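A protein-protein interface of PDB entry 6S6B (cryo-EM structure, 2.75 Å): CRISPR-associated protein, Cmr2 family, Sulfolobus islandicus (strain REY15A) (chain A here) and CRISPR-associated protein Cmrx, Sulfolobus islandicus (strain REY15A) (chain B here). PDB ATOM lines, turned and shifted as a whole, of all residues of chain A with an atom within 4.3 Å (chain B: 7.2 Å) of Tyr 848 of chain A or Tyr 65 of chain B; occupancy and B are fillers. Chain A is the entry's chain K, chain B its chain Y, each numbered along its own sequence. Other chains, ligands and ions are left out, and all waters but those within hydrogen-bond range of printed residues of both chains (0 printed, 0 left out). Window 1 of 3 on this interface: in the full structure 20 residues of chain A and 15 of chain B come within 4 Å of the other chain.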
ATOM      1  N   ARG A 111      12.407  12.711   3.595  1.00  0.00           N
ATOM      2  CA  ARG A 111      11.074  12.632   4.163  1.00  0.00           C
ATOM      3  C   ARG A 111      11.217  12.125   5.587  1.00  0.00           C
ATOM      4  O   ARG A 111      12.304  11.734   6.020  1.00  0.00           O
ATOM      5  CB  ARG A 111      10.161  11.712   3.350  1.00  0.00           C
ATOM      6  CG  ARG A 111       9.988  12.144   1.920  1.00  0.00           C
ATOM      7  CD  ARG A 111       9.545  13.585   1.845  1.00  0.00           C
ATOM      8  NE  ARG A 111       8.213  13.773   2.403  1.00  0.00           N
ATOM      9  CZ  ARG A 111       7.385  14.741   2.031  1.00  0.00           C
ATOM     10  NH1 ARG A 111       7.753  15.606   1.098  1.00  0.00           N
ATOM     11  NH2 ARG A 111       6.187  14.844   2.588  1.00  0.00           N
ATOM     12  N   ASN A 165       6.911   4.094   3.672  1.00  0.00           N
ATOM     13  CA  ASN A 165       8.086   3.386   3.190  1.00  0.00           C
ATOM     14  C   ASN A 165       9.305   3.787   4.009  1.00  0.00           C
ATOM     15  O   ASN A 165       9.533   4.970   4.269  1.00  0.00           O
ATOM     16  CB  ASN A 165       8.317   3.690   1.713  1.00  0.00           C
ATOM     17  CG  ASN A 165       9.098   2.608   1.017  1.00  0.00           C
ATOM     18  OD1 ASN A 165       9.940   1.947   1.619  1.00  0.00           O
ATOM     19  ND2 ASN A 165       8.819   2.415  -0.263  1.00  0.00           N
ATOM     20  N   THR A 176      15.642   2.772  -0.053  1.00  0.00           N
ATOM     21  CA  THR A 176      14.379   2.219   0.410  1.00  0.00           C
ATOM     22  C   THR A 176      14.526   0.731   0.683  1.00  0.00           C
ATOM     23  O   THR A 176      15.187   0.011  -0.069  1.00  0.00           O
ATOM     24  CB  THR A 176      13.281   2.456  -0.620  1.00  0.00           C
ATOM     25  OG1 THR A 176      13.761   2.090  -1.917  1.00  0.00           O
ATOM     26  CG2 THR A 176      12.876   3.913  -0.632  1.00  0.00           C
ATOM     27  N   GLU A 838       6.069  15.037  -4.506  1.00  0.00           N
ATOM     28  CA  GLU A 838       6.421  15.750  -3.278  1.00  0.00           C
ATOM     29  C   GLU A 838       7.904  16.097  -3.284  1.00  0.00           C
ATOM     30  O   GLU A 838       8.712  15.384  -2.687  1.00  0.00           O
ATOM     31  CB  GLU A 838       6.060  14.903  -2.056  1.00  0.00           C
ATOM     32  CG  GLU A 838       4.596  14.952  -1.664  1.00  0.00           C
ATOM     33  CD  GLU A 838       3.784  13.862  -2.327  1.00  0.00           C
ATOM     34  OE1 GLU A 838       4.274  13.272  -3.311  1.00  0.00           O
ATOM     35  OE2 GLU A 838       2.661  13.590  -1.857  1.00  0.00           O
ATOM     36  N   PHE A 841      10.062  13.406  -4.505  1.00  0.00           N
ATOM     37  CA  PHE A 841       9.671  12.154  -3.868  1.00  0.00           C
ATOM     38  C   PHE A 841       8.253  11.828  -4.332  1.00  0.00           C
ATOM     39  O   PHE A 841       7.292  12.413  -3.831  1.00  0.00           O
ATOM     40  CB  PHE A 841       9.742  12.261  -2.357  1.00  0.00           C
ATOM     41  CG  PHE A 841      11.050  11.838  -1.783  1.00  0.00           C
ATOM     42  CD1 PHE A 841      11.383  10.503  -1.712  1.00  0.00           C
ATOM     43  CD2 PHE A 841      11.943  12.773  -1.300  1.00  0.00           C
ATOM     44  CE1 PHE A 841      12.583  10.109  -1.182  1.00  0.00           C
ATOM     45  CE2 PHE A 841      13.147  12.385  -0.768  1.00  0.00           C
ATOM     46  CZ  PHE A 841      13.468  11.051  -0.706  1.00  0.00           C
ATOM     47  N   VAL A 842       8.137  10.903  -5.281  1.00  0.00           N
ATOM     48  CA  VAL A 842       6.820  10.421  -5.669  1.00  0.00           C
ATOM     49  C   VAL A 842       6.249   9.593  -4.527  1.00  0.00           C
ATOM     50  O   VAL A 842       6.930   8.731  -3.958  1.00  0.00           O
ATOM     51  CB  VAL A 842       6.894   9.629  -6.984  1.00  0.00           C
ATOM     52  CG1 VAL A 842       7.891   8.493  -6.881  1.00  0.00           C
ATOM     53  CG2 VAL A 842       5.525   9.105  -7.364  1.00  0.00           C
ATOM     54  N   ARG A 843       5.003   9.878  -4.158  1.00  0.00           N
ATOM     55  CA  ARG A 843       4.367   9.266  -2.999  1.00  0.00           C
ATOM     56  C   ARG A 843       3.105   8.548  -3.443  1.00  0.00           C
ATOM     57  O   ARG A 843       2.228   9.156  -4.063  1.00  0.00           O
ATOM     58  CB  ARG A 843       4.033  10.312  -1.937  1.00  0.00           C
ATOM     59  CG  ARG A 843       3.066   9.814  -0.885  1.00  0.00           C
ATOM     60  CD  ARG A 843       2.896  10.810   0.246  1.00  0.00           C
ATOM     61  NE  ARG A 843       1.983  11.896  -0.094  1.00  0.00           N
ATOM     62  CZ  ARG A 843       0.662  11.770  -0.156  1.00  0.00           C
ATOM     63  NH1 ARG A 843       0.091  10.602   0.096  1.00  0.00           N
ATOM     64  NH2 ARG A 843      -0.089  12.816  -0.469  1.00  0.00           N
ATOM     65  N   ASN A 846       1.116   7.272   1.199  1.00  0.00           N
ATOM     66  CA  ASN A 846       1.999   7.386   2.356  1.00  0.00           C
ATOM     67  C   ASN A 846       3.348   6.719   2.113  1.00  0.00           C
ATOM     68  O   ASN A 846       4.256   6.836   2.940  1.00  0.00           O
ATOM     69  CB  ASN A 846       1.352   6.795   3.614  1.00  0.00           C
ATOM     70  CG  ASN A 846      -0.105   7.172   3.753  1.00  0.00           C
ATOM     71  OD1 ASN A 846      -0.992   6.352   3.528  1.00  0.00           O
ATOM     72  ND2 ASN A 846      -0.360   8.418   4.128  1.00  0.00           N
ATOM     73  N   ALA A 847       3.498   6.032   0.986  1.00  0.00           N
ATOM     74  CA  ALA A 847       4.751   5.371   0.643  1.00  0.00           C
ATOM     75  C   ALA A 847       5.575   6.321  -0.212  1.00  0.00           C
ATOM     76  O   ALA A 847       5.194   6.639  -1.342  1.00  0.00           O
ATOM     77  CB  ALA A 847       4.489   4.057  -0.085  1.00  0.00           C
ATOM     78  N   TYR A 848       6.705   6.772   0.324  1.00  0.00           N
ATOM     79  CA  TYR A 848       7.557   7.724  -0.369  1.00  0.00           C
ATOM     80  C   TYR A 848       8.613   6.988  -1.177  1.00  0.00           C
ATOM     81  O   TYR A 848       9.292   6.095  -0.661  1.00  0.00           O
ATOM     82  CB  TYR A 848       8.220   8.675   0.623  1.00  0.00           C
ATOM     83  CG  TYR A 848       7.324   9.805   1.044  1.00  0.00           C
ATOM     84  CD1 TYR A 848       7.082  10.870   0.195  1.00  0.00           C
ATOM     85  CD2 TYR A 848       6.715   9.805   2.285  1.00  0.00           C
ATOM     86  CE1 TYR A 848       6.260  11.905   0.569  1.00  0.00           C
ATOM     87  CE2 TYR A 848       5.891  10.838   2.670  1.00  0.00           C
ATOM     88  CZ  TYR A 848       5.668  11.886   1.808  1.00  0.00           C
ATOM     89  OH  TYR A 848       4.847  12.921   2.182  1.00  0.00           O
ATOM     90  N   TYR A 849       8.749   7.368  -2.443  1.00  0.00           N
ATOM     91  CA  TYR A 849       9.717   6.768  -3.338  1.00  0.00           C
ATOM     92  C   TYR A 849      10.577   7.856  -3.964  1.00  0.00           C
ATOM     93  O   TYR A 849      10.067   8.922  -4.325  1.00  0.00           O
ATOM     94  CB  TYR A 849       9.017   5.965  -4.434  1.00  0.00           C
ATOM     95  CG  TYR A 849       8.812   4.514  -4.086  1.00  0.00           C
ATOM     96  CD1 TYR A 849       9.864   3.737  -3.632  1.00  0.00           C
ATOM     97  CD2 TYR A 849       7.565   3.924  -4.204  1.00  0.00           C
ATOM     98  CE1 TYR A 849       9.683   2.415  -3.315  1.00  0.00           C
ATOM     99  CE2 TYR A 849       7.376   2.602  -3.888  1.00  0.00           C
ATOM    100  CZ  TYR A 849       8.436   1.853  -3.443  1.00  0.00           C
ATOM    101  OH  TYR A 849       8.250   0.530  -3.124  1.00  0.00           O
ATOM    102  N   TYR B   7      -4.096  23.006  18.429  1.00  0.00           N
ATOM    103  CA  TYR B   7      -3.313  22.640  17.245  1.00  0.00           C
ATOM    104  C   TYR B   7      -3.137  23.891  16.386  1.00  0.00           C
ATOM    105  O   TYR B   7      -3.984  24.206  15.548  1.00  0.00           O
ATOM    106  CB  TYR B   7      -3.997  21.518  16.475  1.00  0.00           C
ATOM    107  CG  TYR B   7      -3.422  21.261  15.102  1.00  0.00           C
ATOM    108  CD1 TYR B   7      -2.059  21.360  14.864  1.00  0.00           C
ATOM    109  CD2 TYR B   7      -4.247  20.933  14.037  1.00  0.00           C
ATOM    110  CE1 TYR B   7      -1.537  21.135  13.613  1.00  0.00           C
ATOM    111  CE2 TYR B   7      -3.729  20.710  12.781  1.00  0.00           C
ATOM    112  CZ  TYR B   7      -2.374  20.809  12.575  1.00  0.00           C
ATOM    113  OH  TYR B   7      -1.852  20.583  11.326  1.00  0.00           O
ATOM    114  N   VAL B  43       0.348  15.594  12.360  1.00  0.00           N
ATOM    115  CA  VAL B  43      -0.094  15.721  10.967  1.00  0.00           C
ATOM    116  C   VAL B  43      -1.503  15.153  10.860  1.00  0.00           C
ATOM    117  O   VAL B  43      -1.700  13.941  11.016  1.00  0.00           O
ATOM    118  CB  VAL B  43       0.847  15.003   9.998  1.00  0.00           C
ATOM    119  CG1 VAL B  43       0.520  15.373   8.568  1.00  0.00           C
ATOM    120  CG2 VAL B  43       2.296  15.278  10.333  1.00  0.00           C
ATOM    121  N   ILE B  44      -2.482  16.020  10.588  1.00  0.00           N
ATOM    122  CA  ILE B  44      -3.821  15.543  10.266  1.00  0.00           C
ATOM    123  C   ILE B  44      -3.819  14.933   8.872  1.00  0.00           C
ATOM    124  O   ILE B  44      -3.197  15.464   7.941  1.00  0.00           O
ATOM    125  CB  ILE B  44      -4.853  16.680  10.362  1.00  0.00           C
ATOM    126  CG1 ILE B  44      -5.050  17.126  11.805  1.00  0.00           C
ATOM    127  CG2 ILE B  44      -6.181  16.262   9.754  1.00  0.00           C
ATOM    128  CD1 ILE B  44      -5.951  18.326  11.923  1.00  0.00           C
ATOM    129  N   THR B  45      -4.518  13.814   8.722  1.00  0.00           N
ATOM    130  CA  THR B  45      -4.678  13.151   7.435  1.00  0.00           C
ATOM    131  C   THR B  45      -6.035  13.506   6.840  1.00  0.00           C
ATOM    132  O   THR B  45      -7.066  13.359   7.502  1.00  0.00           O
ATOM    133  CB  THR B  45      -4.550  11.635   7.585  1.00  0.00           C
ATOM    134  OG1 THR B  45      -3.404  11.330   8.389  1.00  0.00           O
ATOM    135  CG2 THR B  45      -4.406  10.969   6.224  1.00  0.00           C
ATOM    136  N   GLY B  46      -6.030  13.975   5.594  1.00  0.00           N
ATOM    137  CA  GLY B  46      -7.264  14.213   4.877  1.00  0.00           C
ATOM    138  C   GLY B  46      -7.878  15.579   5.060  1.00  0.00           C
ATOM    139  O   GLY B  46      -9.109  15.694   5.067  1.00  0.00           O
ATOM    140  N   TYR B  47      -7.069  16.624   5.204  1.00  0.00           N
ATOM    141  CA  TYR B  47      -7.569  17.973   5.411  1.00  0.00           C
ATOM    142  C   TYR B  47      -6.877  18.940   4.465  1.00  0.00           C
ATOM    143  O   TYR B  47      -5.771  18.689   3.981  1.00  0.00           O
ATOM    144  CB  TYR B  47      -7.361  18.437   6.858  1.00  0.00           C
ATOM    145  CG  TYR B  47      -8.537  18.169   7.765  1.00  0.00           C
ATOM    146  CD1 TYR B  47      -9.042  16.887   7.918  1.00  0.00           C
ATOM    147  CD2 TYR B  47      -9.143  19.201   8.470  1.00  0.00           C
ATOM    148  CE1 TYR B  47     -10.113  16.635   8.748  1.00  0.00           C
ATOM    149  CE2 TYR B  47     -10.218  18.961   9.302  1.00  0.00           C
ATOM    150  CZ  TYR B  47     -10.699  17.674   9.436  1.00  0.00           C
ATOM    151  OH  TYR B  47     -11.769  17.422  10.261  1.00  0.00           O
ATOM    152  N   ALA B  48      -7.548  20.057   4.209  1.00  0.00           N
ATOM    153  CA  ALA B  48      -6.981  21.165   3.464  1.00  0.00           C
ATOM    154  C   ALA B  48      -6.464  22.215   4.439  1.00  0.00           C
ATOM    155  O   ALA B  48      -6.456  22.022   5.656  1.00  0.00           O
ATOM    156  CB  ALA B  48      -8.016  21.763   2.512  1.00  0.00           C
ATOM    157  N   VAL B  49      -6.022  23.346   3.893  1.00  0.00           N
ATOM    158  CA  VAL B  49      -5.510  24.443   4.707  1.00  0.00           C
ATOM    159  C   VAL B  49      -6.211  25.726   4.278  1.00  0.00           C
ATOM    160  O   VAL B  49      -6.216  26.723   5.009  1.00  0.00           O
ATOM    161  CB  VAL B  49      -3.975  24.536   4.592  1.00  0.00           C
ATOM    162  CG1 VAL B  49      -3.425  25.788   5.274  1.00  0.00           C
ATOM    163  CG2 VAL B  49      -3.338  23.288   5.187  1.00  0.00           C
ATOM    164  N   ASP B  61     -10.178  12.417   0.833  1.00  0.00           N
ATOM    165  CA  ASP B  61      -9.197  11.434   0.387  1.00  0.00           C
ATOM    166  C   ASP B  61      -8.074  11.307   1.403  1.00  0.00           C
ATOM    167  O   ASP B  61      -7.544  12.326   1.869  1.00  0.00           O
ATOM    168  CB  ASP B  61      -8.625  11.800  -0.979  1.00  0.00           C
ATOM    169  CG  ASP B  61      -8.065  13.199  -1.024  1.00  0.00           C
ATOM    170  OD1 ASP B  61      -8.299  13.977  -0.081  1.00  0.00           O
ATOM    171  OD2 ASP B  61      -7.359  13.516  -1.998  1.00  0.00           O
ATOM    172  N   PRO B  62      -7.690  10.090   1.777  1.00  0.00           N
ATOM    173  CA  PRO B  62      -6.582   9.875   2.717  1.00  0.00           C
ATOM    174  C   PRO B  62      -5.216  10.122   2.080  1.00  0.00           C
ATOM    175  O   PRO B  62      -4.307   9.296   2.173  1.00  0.00           O
ATOM    176  CB  PRO B  62      -6.767   8.411   3.125  1.00  0.00           C
ATOM    177  CG  PRO B  62      -7.394   7.777   1.929  1.00  0.00           C
ATOM    178  CD  PRO B  62      -8.289   8.824   1.322  1.00  0.00           C
ATOM    179  N   CYS B  63      -5.076  11.273   1.426  1.00  0.00           N
ATOM    180  CA  CYS B  63      -3.875  11.624   0.690  1.00  0.00           C
ATOM    181  C   CYS B  63      -3.246  12.926   1.165  1.00  0.00           C
ATOM    182  O   CYS B  63      -2.112  13.229   0.777  1.00  0.00           O
ATOM    183  CB  CYS B  63      -4.202  11.719  -0.807  1.00  0.00           C
ATOM    184  SG  CYS B  63      -2.804  12.039  -1.894  1.00  0.00           S
ATOM    185  N   ASP B  64      -3.931  13.688   2.011  1.00  0.00           N
ATOM    186  CA  ASP B  64      -3.500  15.025   2.387  1.00  0.00           C
ATOM    187  C   ASP B  64      -2.761  15.014   3.718  1.00  0.00           C
ATOM    188  O   ASP B  64      -2.972  14.143   4.565  1.00  0.00           O
ATOM    189  CB  ASP B  64      -4.699  15.967   2.468  1.00  0.00           C
ATOM    190  CG  ASP B  64      -5.607  15.843   1.272  1.00  0.00           C
ATOM    191  OD1 ASP B  64      -5.104  15.933   0.136  1.00  0.00           O
ATOM    192  OD2 ASP B  64      -6.821  15.648   1.465  1.00  0.00           O
ATOM    193  N   TYR B  65      -1.884  15.999   3.889  1.00  0.00           N
ATOM    194  CA  TYR B  65      -1.138  16.190   5.122  1.00  0.00           C
ATOM    195  C   TYR B  65      -1.281  17.637   5.559  1.00  0.00           C
ATOM    196  O   TYR B  65      -0.976  18.552   4.789  1.00  0.00           O
ATOM    197  CB  TYR B  65       0.344  15.845   4.947  1.00  0.00           C
ATOM    198  CG  TYR B  65       0.604  14.407   4.577  1.00  0.00           C
ATOM    199  CD1 TYR B  65       0.398  13.389   5.497  1.00  0.00           C
ATOM    200  CD2 TYR B  65       1.060  14.066   3.311  1.00  0.00           C
ATOM    201  CE1 TYR B  65       0.632  12.070   5.165  1.00  0.00           C
ATOM    202  CE2 TYR B  65       1.300  12.750   2.971  1.00  0.00           C
ATOM    203  CZ  TYR B  65       1.083  11.756   3.902  1.00  0.00           C
ATOM    204  OH  TYR B  65       1.319  10.444   3.566  1.00  0.00           O
ATOM    205  N   VAL B  66      -1.750  17.839   6.785  1.00  0.00           N
ATOM    206  CA  VAL B  66      -1.776  19.151   7.415  1.00  0.00           C
ATOM    207  C   VAL B  66      -0.996  19.039   8.712  1.00  0.00           C
ATOM    208  O   VAL B  66      -1.413  18.328   9.635  1.00  0.00           O
ATOM    209  CB  VAL B  66      -3.209  19.641   7.665  1.00  0.00           C
ATOM    210  CG1 VAL B  66      -3.186  20.949   8.420  1.00  0.00           C
ATOM    211  CG2 VAL B  66      -3.937  19.806   6.344  1.00  0.00           C
ATOM    212  N   LYS B  67       0.139  19.727   8.782  1.00  0.00           N
ATOM    213  CA  LYS B  67       1.093  19.528   9.858  1.00  0.00           C
ATOM    214  C   LYS B  67       1.190  20.769  10.734  1.00  0.00           C
ATOM    215  O   LYS B  67       0.873  21.886  10.318  1.00  0.00           O
ATOM    216  CB  LYS B  67       2.473  19.165   9.302  1.00  0.00           C
ATOM    217  CG  LYS B  67       2.413  18.298   8.061  1.00  0.00           C
ATOM    218  CD  LYS B  67       3.660  17.453   7.913  1.00  0.00           C
ATOM    219  CE  LYS B  67       3.695  16.747   6.569  1.00  0.00           C
ATOM    220  NZ  LYS B  67       4.877  15.855   6.456  1.00  0.00           N
ATOM    221  N   TYR B  94      -1.506  10.493  13.816  1.00  0.00           N
ATOM    222  CA  TYR B  94      -0.397  10.442  12.873  1.00  0.00           C
ATOM    223  C   TYR B  94       0.669  11.389  13.411  1.00  0.00           C
ATOM    224  O   TYR B  94       0.547  12.610  13.268  1.00  0.00           O
ATOM    225  CB  TYR B  94      -0.851  10.864  11.477  1.00  0.00           C
ATOM    226  CG  TYR B  94       0.199  10.711  10.403  1.00  0.00           C
ATOM    227  CD1 TYR B  94       0.394   9.502   9.764  1.00  0.00           C
ATOM    228  CD2 TYR B  94       1.018  11.769  10.049  1.00  0.00           C
ATOM    229  CE1 TYR B  94       1.357   9.359   8.782  1.00  0.00           C
ATOM    230  CE2 TYR B  94       1.987  11.637   9.072  1.00  0.00           C
ATOM    231  CZ  TYR B  94       2.150  10.424   8.442  1.00  0.00           C
ATOM    232  OH  TYR B  94       3.111  10.283   7.469  1.00  0.00           O
ATOM    233  N   THR B 123      -6.701  20.449  -3.936  1.00  0.00           N
ATOM    234  CA  THR B 123      -5.529  20.279  -3.087  1.00  0.00           C
ATOM    235  C   THR B 123      -4.313  20.848  -3.803  1.00  0.00           C
ATOM    236  O   THR B 123      -4.056  20.511  -4.962  1.00  0.00           O
ATOM    237  CB  THR B 123      -5.309  18.804  -2.748  1.00  0.00           C
ATOM    238  OG1 THR B 123      -6.315  18.369  -1.826  1.00  0.00           O
ATOM    239  CG2 THR B 123      -3.942  18.589  -2.130  1.00  0.00           C
ATOM    240  N   VAL B 126       2.359  22.546  -1.149  1.00  0.00           N
ATOM    241  CA  VAL B 126       3.044  23.770  -0.754  1.00  0.00           C
ATOM    242  C   VAL B 126       3.858  23.489   0.502  1.00  0.00           C
ATOM    243  O   VAL B 126       3.499  22.631   1.313  1.00  0.00           O
ATOM    244  CB  VAL B 126       2.026  24.921  -0.548  1.00  0.00           C
ATOM    245  CG1 VAL B 126       1.003  24.529   0.496  1.00  0.00           C
ATOM    246  CG2 VAL B 126       2.730  26.219  -0.169  1.00  0.00           C
ATOM    247  N   PHE B 167       6.980  20.440   8.364  1.00  0.00           N
ATOM    248  CA  PHE B 167       5.598  20.869   8.162  1.00  0.00           C
ATOM    249  C   PHE B 167       5.390  21.192   6.688  1.00  0.00           C
ATOM    250  O   PHE B 167       5.746  22.276   6.220  1.00  0.00           O
ATOM    251  CB  PHE B 167       5.283  22.069   9.047  1.00  0.00           C
ATOM    252  CG  PHE B 167       5.676  21.880  10.485  1.00  0.00           C
ATOM    253  CD1 PHE B 167       6.930  22.270  10.927  1.00  0.00           C
ATOM    254  CD2 PHE B 167       4.804  21.306  11.393  1.00  0.00           C
ATOM    255  CE1 PHE B 167       7.304  22.097  12.247  1.00  0.00           C
ATOM    256  CE2 PHE B 167       5.173  21.132  12.714  1.00  0.00           C
ATOM    257  CZ  PHE B 167       6.425  21.527  13.139  1.00  0.00           C
ATOM    258  N   SER B 168       4.817  20.244   5.952  1.00  0.00           N
ATOM    259  CA  SER B 168       4.422  20.443   4.563  1.00  0.00           C
ATOM    260  C   SER B 168       2.926  20.197   4.456  1.00  0.00           C
ATOM    261  O   SER B 168       2.458  19.082   4.709  1.00  0.00           O
ATOM    262  CB  SER B 168       5.201  19.519   3.626  1.00  0.00           C
ATOM    263  OG  SER B 168       4.900  18.158   3.875  1.00  0.00           O
ATOM    264  N   TYR B 169       2.183  21.231   4.085  1.00  0.00           N
ATOM    265  CA  TYR B 169       0.728  21.207   4.071  1.00  0.00           C
ATOM    266  C   TYR B 169       0.211  21.227   2.636  1.00  0.00           C
ATOM    267  O   TYR B 169       0.976  21.316   1.672  1.00  0.00           O
ATOM    268  CB  TYR B 169       0.170  22.379   4.880  1.00  0.00           C
ATOM    269  CG  TYR B 169       0.543  23.744   4.352  1.00  0.00           C
ATOM    270  CD1 TYR B 169       1.856  24.193   4.384  1.00  0.00           C
ATOM    271  CD2 TYR B 169      -0.424  24.592   3.839  1.00  0.00           C
ATOM    272  CE1 TYR B 169       2.195  25.440   3.903  1.00  0.00           C
ATOM    273  CE2 TYR B 169      -0.099  25.842   3.364  1.00  0.00           C
ATOM    274  CZ  TYR B 169       1.212  26.262   3.396  1.00  0.00           C
ATOM    275  OH  TYR B 169       1.538  27.508   2.916  1.00  0.00           O
ATOM    276  N   TYR B 170      -1.111  21.138   2.500  1.00  0.00           N
ATOM    277  CA  TYR B 170      -1.769  21.061   1.199  1.00  0.00           C
ATOM    278  C   TYR B 170      -2.778  22.196   1.096  1.00  0.00           C
ATOM    279  O   TYR B 170      -3.775  22.210   1.825  1.00  0.00           O
ATOM    280  CB  TYR B 170      -2.442  19.703   1.011  1.00  0.00           C
ATOM    281  CG  TYR B 170      -1.506  18.635   0.494  1.00  0.00           C
ATOM    282  CD1 TYR B 170      -0.816  18.805  -0.696  1.00  0.00           C
ATOM    283  CD2 TYR B 170      -1.302  17.462   1.205  1.00  0.00           C
ATOM    284  CE1 TYR B 170       0.041  17.832  -1.169  1.00  0.00           C
ATOM    285  CE2 TYR B 170      -0.445  16.483   0.741  1.00  0.00           C
ATOM    286  CZ  TYR B 170       0.223  16.675  -0.447  1.00  0.00           C
ATOM    287  OH  TYR B 170       1.077  15.705  -0.915  1.00  0.00           O
ATOM    288  N   ALA B 171      -2.529  23.132   0.181  1.00  0.00           N
ATOM    289  CA  ALA B 171      -3.317  24.354   0.073  1.00  0.00           C
ATOM    290  C   ALA B 171      -4.623  24.081  -0.676  1.00  0.00           C
ATOM    291  O   ALA B 171      -4.998  22.934  -0.935  1.00  0.00           O
ATOM    292  CB  ALA B 171      -2.488  25.450  -0.587  1.00  0.00           C
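NE of Arg 111 of chain A lies close to OH of Tyr 848 of chain A (3.5 Å). NE of Arg 843 of chain A lies within salt-bridge range of OE2 of Glu 838 of chain A (2.5 Å). O of Tyr 170 of chain B sits at hydrogen-bond distance from N of Val 49 of chain B (3.3 Å). N of Tyr 170 of chain B sits at hydrogen-bond distance from O of Tyr 65 of chain B, 3.5 Å away. The side-chain amino group of Lys 67 of chain B sits close to the side-chain hydroxyl of Ser 168 of chain B (3.5 Å).
Of the 23 printed residues of chain B, 4 touch a printed residue of chain A. Of the 11 printed residues of chain A, 5 touch a printed residue of chain B. Among the printed residues, no Asp or Glu carboxylate lies within 4 Å of a Lys or Arg side-chain nitrogen of the other chain.
OE2 of Glu 838 of chain A sits at hydrogen-bond distance from OH of Tyr 170 of chain B, at 2.8 Å. O of Cys 63 of chain B is in hydrogen-bond range of NH2 of Arg 843 of chain A. NH2 of Arg 843 of chain A sits at hydrogen-bond distance from OH of Tyr 170 of chain B, 3.1 Å away. ND2 of Asn 846 of chain A lies within hydrogen-bond range of OH of Tyr 65 of chain B (2.7 Å).
Tyr 848 of chain A touches just one residue of chain B: Tyr 65 (3.6 Å). Tyr 65 of chain B touches three residues of chain A. Of the printed residues of chain B, Arg 843 of chain A touches Cys 63, Tyr 65 and Tyr 170. Printed residues of chain B within 4 Å of Arg 111 of chain A: Ser 168. Printed residues of chain B within 4 Å of Asn 846 of chain A: Tyr 65 (2.7 Å). Printed residues of chain B within 4 Å of Glu 838 of chain A: Tyr 170. Printed residues of chain A within 4 Å of Ser 168 of chain B: Arg 111 (3.8 Å). Tyr 94 of chain B touches none of the printed residues of chain A. Tyr 849 of chain A touches none of the printed residues of chain B. The nearest residue of chain B that does not touch Tyr 848 of chain A is Lys 67 of chain B (5.2 Å). The nearest printed residue of chain A that does not touch Tyr 65 of chain B is Glu 838 of chain A (5.1 Å). The nearest printed residue of chain B that does not touch Glu 838 of chain A is Tyr 65 of chain B (5.1 Å).
Among the printed residues, pairs that only touch across the chains: Arg 111 of chain A with Ser 168 of chain B (3.8 Å), Arg 843 of chain A with Tyr 65 of chain B (3.3 Å) and Tyr 848 of chain A with Tyr 65 of chain B (3.6 Å).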
